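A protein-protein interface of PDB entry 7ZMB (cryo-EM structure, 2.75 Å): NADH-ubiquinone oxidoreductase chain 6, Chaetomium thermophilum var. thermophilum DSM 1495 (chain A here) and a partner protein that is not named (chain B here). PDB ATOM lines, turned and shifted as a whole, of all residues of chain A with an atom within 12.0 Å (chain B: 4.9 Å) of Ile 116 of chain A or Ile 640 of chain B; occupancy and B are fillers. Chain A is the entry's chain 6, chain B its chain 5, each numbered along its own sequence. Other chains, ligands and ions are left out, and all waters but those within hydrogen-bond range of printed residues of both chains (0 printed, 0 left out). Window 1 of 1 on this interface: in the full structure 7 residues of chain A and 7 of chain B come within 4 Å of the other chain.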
ATOM      1  N   ILE A 107      14.111  -4.833  43.696  1.00  0.00           N
ATOM      2  CA  ILE A 107      13.252  -5.309  42.618  1.00  0.00           C
ATOM      3  C   ILE A 107      13.169  -4.296  41.479  1.00  0.00           C
ATOM      4  O   ILE A 107      13.291  -4.700  40.315  1.00  0.00           O
ATOM      5  CB  ILE A 107      11.851  -5.664  43.138  1.00  0.00           C
ATOM      6  CG1 ILE A 107      11.951  -6.748  44.206  1.00  0.00           C
ATOM      7  CG2 ILE A 107      10.947  -6.116  41.999  1.00  0.00           C
ATOM      8  CD1 ILE A 107      12.555  -8.034  43.701  1.00  0.00           C
ATOM      9  N   PRO A 108      12.942  -2.995  41.728  1.00  0.00           N
ATOM     10  CA  PRO A 108      12.854  -2.073  40.582  1.00  0.00           C
ATOM     11  C   PRO A 108      14.130  -2.002  39.769  1.00  0.00           C
ATOM     12  O   PRO A 108      14.074  -1.836  38.548  1.00  0.00           O
ATOM     13  CB  PRO A 108      12.508  -0.723  41.225  1.00  0.00           C
ATOM     14  CG  PRO A 108      12.191  -1.002  42.633  1.00  0.00           C
ATOM     15  CD  PRO A 108      12.803  -2.285  43.010  1.00  0.00           C
ATOM     16  N   LEU A 109      15.286  -2.123  40.415  1.00  0.00           N
ATOM     17  CA  LEU A 109      16.530  -2.199  39.662  1.00  0.00           C
ATOM     18  C   LEU A 109      16.586  -3.483  38.847  1.00  0.00           C
ATOM     19  O   LEU A 109      17.045  -3.478  37.702  1.00  0.00           O
ATOM     20  CB  LEU A 109      17.720  -2.083  40.616  1.00  0.00           C
ATOM     21  CG  LEU A 109      19.132  -1.962  40.048  1.00  0.00           C
ATOM     22  CD1 LEU A 109      19.971  -1.229  41.048  1.00  0.00           C
ATOM     23  CD2 LEU A 109      19.759  -3.310  39.790  1.00  0.00           C
ATOM     24  N   THR A 110      16.104  -4.589  39.422  1.00  0.00           N
ATOM     25  CA  THR A 110      16.083  -5.872  38.725  1.00  0.00           C
ATOM     26  C   THR A 110      15.322  -5.778  37.409  1.00  0.00           C
ATOM     27  O   THR A 110      15.804  -6.229  36.364  1.00  0.00           O
ATOM     28  CB  THR A 110      15.452  -6.937  39.624  1.00  0.00           C
ATOM     29  OG1 THR A 110      16.046  -6.889  40.928  1.00  0.00           O
ATOM     30  CG2 THR A 110      15.630  -8.313  39.035  1.00  0.00           C
ATOM     31  N   ILE A 111      14.133  -5.177  37.443  1.00  0.00           N
ATOM     32  CA  ILE A 111      13.291  -5.115  36.253  1.00  0.00           C
ATOM     33  C   ILE A 111      13.975  -4.311  35.156  1.00  0.00           C
ATOM     34  O   ILE A 111      14.089  -4.765  34.012  1.00  0.00           O
ATOM     35  CB  ILE A 111      11.913  -4.529  36.604  1.00  0.00           C
ATOM     36  CG1 ILE A 111      11.317  -5.261  37.806  1.00  0.00           C
ATOM     37  CG2 ILE A 111      10.979  -4.611  35.407  1.00  0.00           C
ATOM     38  CD1 ILE A 111      11.085  -6.733  37.565  1.00  0.00           C
ATOM     39  N   LEU A 112      14.449  -3.111  35.491  1.00  0.00           N
ATOM     40  CA  LEU A 112      15.115  -2.267  34.505  1.00  0.00           C
ATOM     41  C   LEU A 112      16.390  -2.920  33.986  1.00  0.00           C
ATOM     42  O   LEU A 112      16.607  -3.010  32.774  1.00  0.00           O
ATOM     43  CB  LEU A 112      15.422  -0.904  35.121  1.00  0.00           C
ATOM     44  CG  LEU A 112      14.441   0.240  34.864  1.00  0.00           C
ATOM     45  CD1 LEU A 112      14.861   1.460  35.659  1.00  0.00           C
ATOM     46  CD2 LEU A 112      14.364   0.571  33.380  1.00  0.00           C
ATOM     47  N   VAL A 113      17.248  -3.385  34.896  1.00  0.00           N
ATOM     48  CA  VAL A 113      18.490  -4.032  34.484  1.00  0.00           C
ATOM     49  C   VAL A 113      18.204  -5.334  33.746  1.00  0.00           C
ATOM     50  O   VAL A 113      18.915  -5.688  32.799  1.00  0.00           O
ATOM     51  CB  VAL A 113      19.399  -4.257  35.708  1.00  0.00           C
ATOM     52  CG1 VAL A 113      20.537  -5.207  35.377  1.00  0.00           C
ATOM     53  CG2 VAL A 113      19.946  -2.932  36.203  1.00  0.00           C
ATOM     54  N   GLY A 114      17.165  -6.061  34.154  1.00  0.00           N
ATOM     55  CA  GLY A 114      16.822  -7.286  33.454  1.00  0.00           C
ATOM     56  C   GLY A 114      16.403  -7.047  32.015  1.00  0.00           C
ATOM     57  O   GLY A 114      16.907  -7.692  31.096  1.00  0.00           O
ATOM     58  N   ILE A 115      15.479  -6.109  31.801  1.00  0.00           N
ATOM     59  CA  ILE A 115      14.927  -5.921  30.463  1.00  0.00           C
ATOM     60  C   ILE A 115      15.952  -5.282  29.537  1.00  0.00           C
ATOM     61  O   ILE A 115      16.050  -5.640  28.360  1.00  0.00           O
ATOM     62  CB  ILE A 115      13.618  -5.107  30.519  1.00  0.00           C
ATOM     63  CG1 ILE A 115      13.855  -3.705  31.079  1.00  0.00           C
ATOM     64  CG2 ILE A 115      12.568  -5.840  31.339  1.00  0.00           C
ATOM     65  CD1 ILE A 115      12.668  -2.791  30.942  1.00  0.00           C
ATOM     66  N   ILE A 116      16.729  -4.330  30.047  1.00  0.00           N
ATOM     67  CA  ILE A 116      17.612  -3.569  29.174  1.00  0.00           C
ATOM     68  C   ILE A 116      18.732  -4.450  28.636  1.00  0.00           C
ATOM     69  O   ILE A 116      19.050  -4.400  27.442  1.00  0.00           O
ATOM     70  CB  ILE A 116      18.144  -2.327  29.911  1.00  0.00           C
ATOM     71  CG1 ILE A 116      17.118  -1.195  29.806  1.00  0.00           C
ATOM     72  CG2 ILE A 116      19.485  -1.899  29.349  1.00  0.00           C
ATOM     73  CD1 ILE A 116      17.312  -0.092  30.801  1.00  0.00           C
ATOM     74  N   ILE A 117      19.336  -5.280  29.489  1.00  0.00           N
ATOM     75  CA  ILE A 117      20.373  -6.190  29.009  1.00  0.00           C
ATOM     76  C   ILE A 117      19.773  -7.212  28.051  1.00  0.00           C
ATOM     77  O   ILE A 117      20.300  -7.452  26.960  1.00  0.00           O
ATOM     78  CB  ILE A 117      21.089  -6.872  30.188  1.00  0.00           C
ATOM     79  CG1 ILE A 117      21.806  -5.854  31.054  1.00  0.00           C
ATOM     80  CG2 ILE A 117      22.158  -7.782  29.689  1.00  0.00           C
ATOM     81  CD1 ILE A 117      22.311  -6.407  32.350  1.00  0.00           C
ATOM     82  N   SER A 118      18.632  -7.796  28.428  1.00  0.00           N
ATOM     83  CA  SER A 118      18.021  -8.845  27.620  1.00  0.00           C
ATOM     84  C   SER A 118      17.615  -8.333  26.245  1.00  0.00           C
ATOM     85  O   SER A 118      17.781  -9.032  25.240  1.00  0.00           O
ATOM     86  CB  SER A 118      16.814  -9.428  28.348  1.00  0.00           C
ATOM     87  OG  SER A 118      16.003  -8.400  28.872  1.00  0.00           O
ATOM     88  N   SER A 119      17.058  -7.125  26.182  1.00  0.00           N
ATOM     89  CA  SER A 119      16.718  -6.547  24.890  1.00  0.00           C
ATOM     90  C   SER A 119      17.967  -6.328  24.051  1.00  0.00           C
ATOM     91  O   SER A 119      17.971  -6.594  22.844  1.00  0.00           O
ATOM     92  CB  SER A 119      15.965  -5.231  25.083  1.00  0.00           C
ATOM     93  OG  SER A 119      15.932  -4.483  23.882  1.00  0.00           O
ATOM     94  N   PHE A 120      19.042  -5.853  24.679  1.00  0.00           N
ATOM     95  CA  PHE A 120      20.263  -5.561  23.940  1.00  0.00           C
ATOM     96  C   PHE A 120      20.939  -6.830  23.443  1.00  0.00           C
ATOM     97  O   PHE A 120      21.416  -6.879  22.304  1.00  0.00           O
ATOM     98  CB  PHE A 120      21.211  -4.752  24.813  1.00  0.00           C
ATOM     99  CG  PHE A 120      20.788  -3.338  24.992  1.00  0.00           C
ATOM    100  CD1 PHE A 120      19.780  -2.804  24.216  1.00  0.00           C
ATOM    101  CD2 PHE A 120      21.380  -2.543  25.945  1.00  0.00           C
ATOM    102  CE1 PHE A 120      19.384  -1.508  24.380  1.00  0.00           C
ATOM    103  CE2 PHE A 120      20.990  -1.243  26.106  1.00  0.00           C
ATOM    104  CZ  PHE A 120      19.989  -0.726  25.323  1.00  0.00           C
ATOM    105  N   LEU A 121      20.996  -7.863  24.271  1.00  0.00           N
ATOM    106  CA  LEU A 121      21.713  -9.063  23.878  1.00  0.00           C
ATOM    107  C   LEU A 121      20.866 -10.042  23.086  1.00  0.00           C
ATOM    108  O   LEU A 121      21.387 -11.075  22.662  1.00  0.00           O
ATOM    109  CB  LEU A 121      22.305  -9.780  25.093  1.00  0.00           C
ATOM    110  CG  LEU A 121      22.965  -8.988  26.210  1.00  0.00           C
ATOM    111  CD1 LEU A 121      23.223  -9.951  27.339  1.00  0.00           C
ATOM    112  CD2 LEU A 121      24.237  -8.338  25.742  1.00  0.00           C
ATOM    113  N   PHE A 122      19.583  -9.752  22.876  1.00  0.00           N
ATOM    114  CA  PHE A 122      18.763 -10.637  22.060  1.00  0.00           C
ATOM    115  C   PHE A 122      19.134 -10.539  20.589  1.00  0.00           C
ATOM    116  O   PHE A 122      18.939 -11.500  19.837  1.00  0.00           O
ATOM    117  CB  PHE A 122      17.281 -10.325  22.260  1.00  0.00           C
ATOM    118  CG  PHE A 122      16.358 -11.303  21.588  1.00  0.00           C
ATOM    119  CD1 PHE A 122      16.184 -12.574  22.108  1.00  0.00           C
ATOM    120  CD2 PHE A 122      15.664 -10.951  20.444  1.00  0.00           C
ATOM    121  CE1 PHE A 122      15.336 -13.477  21.499  1.00  0.00           C
ATOM    122  CE2 PHE A 122      14.814 -11.851  19.829  1.00  0.00           C
ATOM    123  CZ  PHE A 122      14.650 -13.115  20.358  1.00  0.00           C
ATOM    124  N   LYS A 123      19.662  -9.388  20.183  1.00  0.00           N
ATOM    125  CA  LYS A 123      20.039  -9.200  18.762  1.00  0.00           C
ATOM    126  C   LYS A 123      21.456  -9.727  18.573  1.00  0.00           C
ATOM    127  O   LYS A 123      21.780 -10.151  17.450  1.00  0.00           O
ATOM    128  CB  LYS A 123      19.887  -7.733  18.340  1.00  0.00           C
ATOM    129  CG  LYS A 123      20.834  -6.749  19.013  1.00  0.00           C
ATOM    130  CD  LYS A 123      20.501  -5.301  18.725  1.00  0.00           C
ATOM    131  CE  LYS A 123      21.551  -4.333  19.227  1.00  0.00           C
ATOM    132  NZ  LYS A 123      21.788  -4.474  20.683  1.00  0.00           N
ATOM    133  N   MET A 124      22.263  -9.688  19.629  1.00  0.00           N
ATOM    134  CA  MET A 124      23.664 -10.175  19.560  1.00  0.00           C
ATOM    135  C   MET A 124      23.681 -11.686  19.297  1.00  0.00           C
ATOM    136  O   MET A 124      24.566 -12.130  18.570  1.00  0.00           O
ATOM    137  CB  MET A 124      24.437  -9.791  20.827  1.00  0.00           C
ATOM    138  CG  MET A 124      24.133  -8.387  21.297  1.00  0.00           C
ATOM    139  SD  MET A 124      25.481  -7.608  22.214  1.00  0.00           S
ATOM    140  CE  MET A 124      24.741  -6.034  22.640  1.00  0.00           C
ATOM    141  N   LEU A 125      22.744 -12.447  19.868  1.00  0.00           N
ATOM    142  CA  LEU A 125      22.631 -13.909  19.605  1.00  0.00           C
ATOM    143  C   LEU A 125      22.172 -14.180  18.165  1.00  0.00           C
ATOM    144  O   LEU A 125      21.365 -13.388  17.661  1.00  0.00           O
ATOM    145  CB  LEU A 125      21.669 -14.496  20.632  1.00  0.00           C
ATOM    146  CG  LEU A 125      22.316 -15.305  21.751  1.00  0.00           C
ATOM    147  CD1 LEU A 125      22.979 -14.393  22.768  1.00  0.00           C
ATOM    148  CD2 LEU A 125      21.285 -16.197  22.421  1.00  0.00           C
ATOM    149  N   LEU B 636      28.045  -2.327  36.791  1.00  0.00           N
ATOM    150  CA  LEU B 636      26.899  -2.731  35.983  1.00  0.00           C
ATOM    151  C   LEU B 636      26.139  -1.524  35.457  1.00  0.00           C
ATOM    152  O   LEU B 636      25.616  -1.553  34.340  1.00  0.00           O
ATOM    153  CB  LEU B 636      25.981  -3.637  36.801  1.00  0.00           C
ATOM    154  CG  LEU B 636      24.668  -4.123  36.188  1.00  0.00           C
ATOM    155  CD1 LEU B 636      24.922  -4.863  34.901  1.00  0.00           C
ATOM    156  CD2 LEU B 636      23.954  -5.005  37.165  1.00  0.00           C
ATOM    157  N   VAL B 637      26.063  -0.452  36.242  1.00  0.00           N
ATOM    158  CA  VAL B 637      25.408   0.764  35.777  1.00  0.00           C
ATOM    159  C   VAL B 637      26.168   1.371  34.606  1.00  0.00           C
ATOM    160  O   VAL B 637      25.569   1.774  33.601  1.00  0.00           O
ATOM    161  CB  VAL B 637      25.254   1.761  36.937  1.00  0.00           C
ATOM    162  CG1 VAL B 637      24.868   3.130  36.420  1.00  0.00           C
ATOM    163  CG2 VAL B 637      24.221   1.253  37.898  1.00  0.00           C
ATOM    164  N   GLY B 638      27.494   1.449  34.712  1.00  0.00           N
ATOM    165  CA  GLY B 638      28.280   1.954  33.601  1.00  0.00           C
ATOM    166  C   GLY B 638      28.216   1.040  32.395  1.00  0.00           C
ATOM    167  O   GLY B 638      28.221   1.502  31.251  1.00  0.00           O
ATOM    168  N   PHE B 639      28.159  -0.268  32.635  1.00  0.00           N
ATOM    169  CA  PHE B 639      27.934  -1.211  31.551  1.00  0.00           C
ATOM    170  C   PHE B 639      26.596  -0.953  30.875  1.00  0.00           C
ATOM    171  O   PHE B 639      26.497  -0.986  29.646  1.00  0.00           O
ATOM    172  CB  PHE B 639      28.011  -2.637  32.097  1.00  0.00           C
ATOM    173  CG  PHE B 639      27.898  -3.704  31.049  1.00  0.00           C
ATOM    174  CD1 PHE B 639      28.988  -4.055  30.279  1.00  0.00           C
ATOM    175  CD2 PHE B 639      26.704  -4.370  30.850  1.00  0.00           C
ATOM    176  CE1 PHE B 639      28.893  -5.045  29.329  1.00  0.00           C
ATOM    177  CE2 PHE B 639      26.603  -5.348  29.902  1.00  0.00           C
ATOM    178  CZ  PHE B 639      27.704  -5.689  29.141  1.00  0.00           C
ATOM    179  N   ILE B 640      25.558  -0.676  31.658  1.00  0.00           N
ATOM    180  CA  ILE B 640      24.243  -0.404  31.087  1.00  0.00           C
ATOM    181  C   ILE B 640      24.282   0.863  30.242  1.00  0.00           C
ATOM    182  O   ILE B 640      23.812   0.882  29.101  1.00  0.00           O
ATOM    183  CB  ILE B 640      23.190  -0.292  32.204  1.00  0.00           C
ATOM    184  CG1 ILE B 640      22.877  -1.671  32.761  1.00  0.00           C
ATOM    185  CG2 ILE B 640      21.927   0.355  31.677  1.00  0.00           C
ATOM    186  CD1 ILE B 640      22.537  -2.637  31.701  1.00  0.00           C
ATOM    187  N   LEU B 641      24.855   1.938  30.794  1.00  0.00           N
ATOM    188  CA  LEU B 641      24.811   3.234  30.135  1.00  0.00           C
ATOM    189  C   LEU B 641      25.626   3.255  28.849  1.00  0.00           C
ATOM    190  O   LEU B 641      25.270   3.972  27.911  1.00  0.00           O
ATOM    191  CB  LEU B 641      25.293   4.321  31.096  1.00  0.00           C
ATOM    192  CG  LEU B 641      24.218   4.870  32.039  1.00  0.00           C
ATOM    193  CD1 LEU B 641      24.806   5.335  33.353  1.00  0.00           C
ATOM    194  CD2 LEU B 641      23.464   5.985  31.362  1.00  0.00           C
ATOM    195  N   TYR B 642      26.719   2.490  28.783  1.00  0.00           N
ATOM    196  CA  TYR B 642      27.487   2.415  27.545  1.00  0.00           C
ATOM    197  C   TYR B 642      26.718   1.667  26.468  1.00  0.00           C
ATOM    198  O   TYR B 642      26.819   2.004  25.285  1.00  0.00           O
ATOM    199  CB  TYR B 642      28.839   1.745  27.782  1.00  0.00           C
ATOM    200  CG  TYR B 642      29.918   2.659  28.301  1.00  0.00           C
ATOM    201  CD1 TYR B 642      29.613   3.764  29.074  1.00  0.00           C
ATOM    202  CD2 TYR B 642      31.247   2.408  28.024  1.00  0.00           C
ATOM    203  CE1 TYR B 642      30.609   4.592  29.553  1.00  0.00           C
ATOM    204  CE2 TYR B 642      32.241   3.221  28.503  1.00  0.00           C
ATOM    205  CZ  TYR B 642      31.915   4.312  29.262  1.00  0.00           C
ATOM    206  OH  TYR B 642      32.906   5.130  29.729  1.00  0.00           O
ATOM    207  N   LEU B 643      25.984   0.621  26.852  1.00  0.00           N
ATOM    208  CA  LEU B 643      25.070  -0.020  25.915  1.00  0.00           C
ATOM    209  C   LEU B 643      23.977   0.941  25.472  1.00  0.00           C
ATOM    210  O   LEU B 643      23.691   1.050  24.277  1.00  0.00           O
ATOM    211  CB  LEU B 643      24.456  -1.282  26.531  1.00  0.00           C
ATOM    212  CG  LEU B 643      25.118  -2.667  26.461  1.00  0.00           C
ATOM    213  CD1 LEU B 643      25.254  -3.117  25.017  1.00  0.00           C
ATOM    214  CD2 LEU B 643      26.465  -2.715  27.132  1.00  0.00           C
ATOM    215  N   ILE B 644      23.375   1.668  26.417  1.00  0.00           N
ATOM    216  CA  ILE B 644      22.340   2.639  26.067  1.00  0.00           C
ATOM    217  C   ILE B 644      22.881   3.654  25.075  1.00  0.00           C
ATOM    218  O   ILE B 644      22.239   3.962  24.065  1.00  0.00           O
ATOM    219  CB  ILE B 644      21.794   3.343  27.323  1.00  0.00           C
ATOM    220  CG1 ILE B 644      21.190   2.358  28.311  1.00  0.00           C
ATOM    221  CG2 ILE B 644      20.750   4.367  26.934  1.00  0.00           C
ATOM    222  CD1 ILE B 644      20.043   1.613  27.760  1.00  0.00           C
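Of the 9 printed residues of chain B, 4 touch a printed residue of chain A. Of the 19 printed residues of chain A, 5 touch a printed residue of chain B. Among the printed residues, no Asp or Glu carboxylate lies within 4 Å of a Lys or Arg side-chain nitrogen of the other chain.
O of Phe 120 of chain A sits at hydrogen-bond distance from NZ of Lys 123 of chain A (2.9 Å).
Of chain B, only Ile 640 and Ile 644 come within 4 Å of Ile 116 of chain A. Printed residues of chain A within 4 Å of Ile 640 of chain B: Ile 116 (3.9 Å) and Ile 117 (3.4 Å). Of chain A, only Val 113 and Ile 117 come within 4 Å of Leu 636 of chain B. No residue of chain A comes within 4 Å of Val 637 of chain B. Gly 638 of chain B touches none of the printed residues of chain A. No residue of chain A comes within 4 Å of Phe 639 of chain B. Leu 641 of chain B touches none of the printed residues of chain A. Of chain A, only Ile 116 and Phe 120 come within 4 Å of Ile 644 of chain B. Printed residues of chain B within 4 Å of Phe 120 of chain A: Leu 643 and Ile 644. Printed residues of chain B within 4 Å of Ile 117 of chain A: Leu 636 (3.96 Å) and Ile 640 (3.4 Å). Of the printed residues of chain B, Val 113 of chain A touches Leu 636 (3.9 Å). Of the printed residues of chain B, Met 124 of chain A touches Leu 643 (3.8 Å). The nearest residue of chain A that does not touch Ile 640 of chain B is Phe 120 of chain A (4.6 Å). The nearest printed residue of chain B that does not touch Ile 117 of chain A is Phe 639 of chain B (5.0 Å).
Val 113 of chain A touches Leu 636 of chain B. CG2 of Ile 116 of chain A touches CD1 of Ile 640 of chain B, 3.9 Å away. CG2 of Ile 116 of chain A touches CD1 of Ile 644 of chain B, 3.9 Å away. CD1 of Leu 636 of chain B touches CD1 of Ile 117 of chain A, at 3.96 Å. Ile 640 of chain B touches Ile 117 of chain A (CD1 to CG1, 3.4 Å). Leu 643 of chain B touches Phe 120 of chain A (CB to CD2, 3.4 Å). CZ of Phe 120 of chain A touches CD1 of Ile 644 of chain B, 3.4 Å away. CE of Met 124 of chain A touches CD1 of Leu 643 of chain B, at 3.8 Å.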
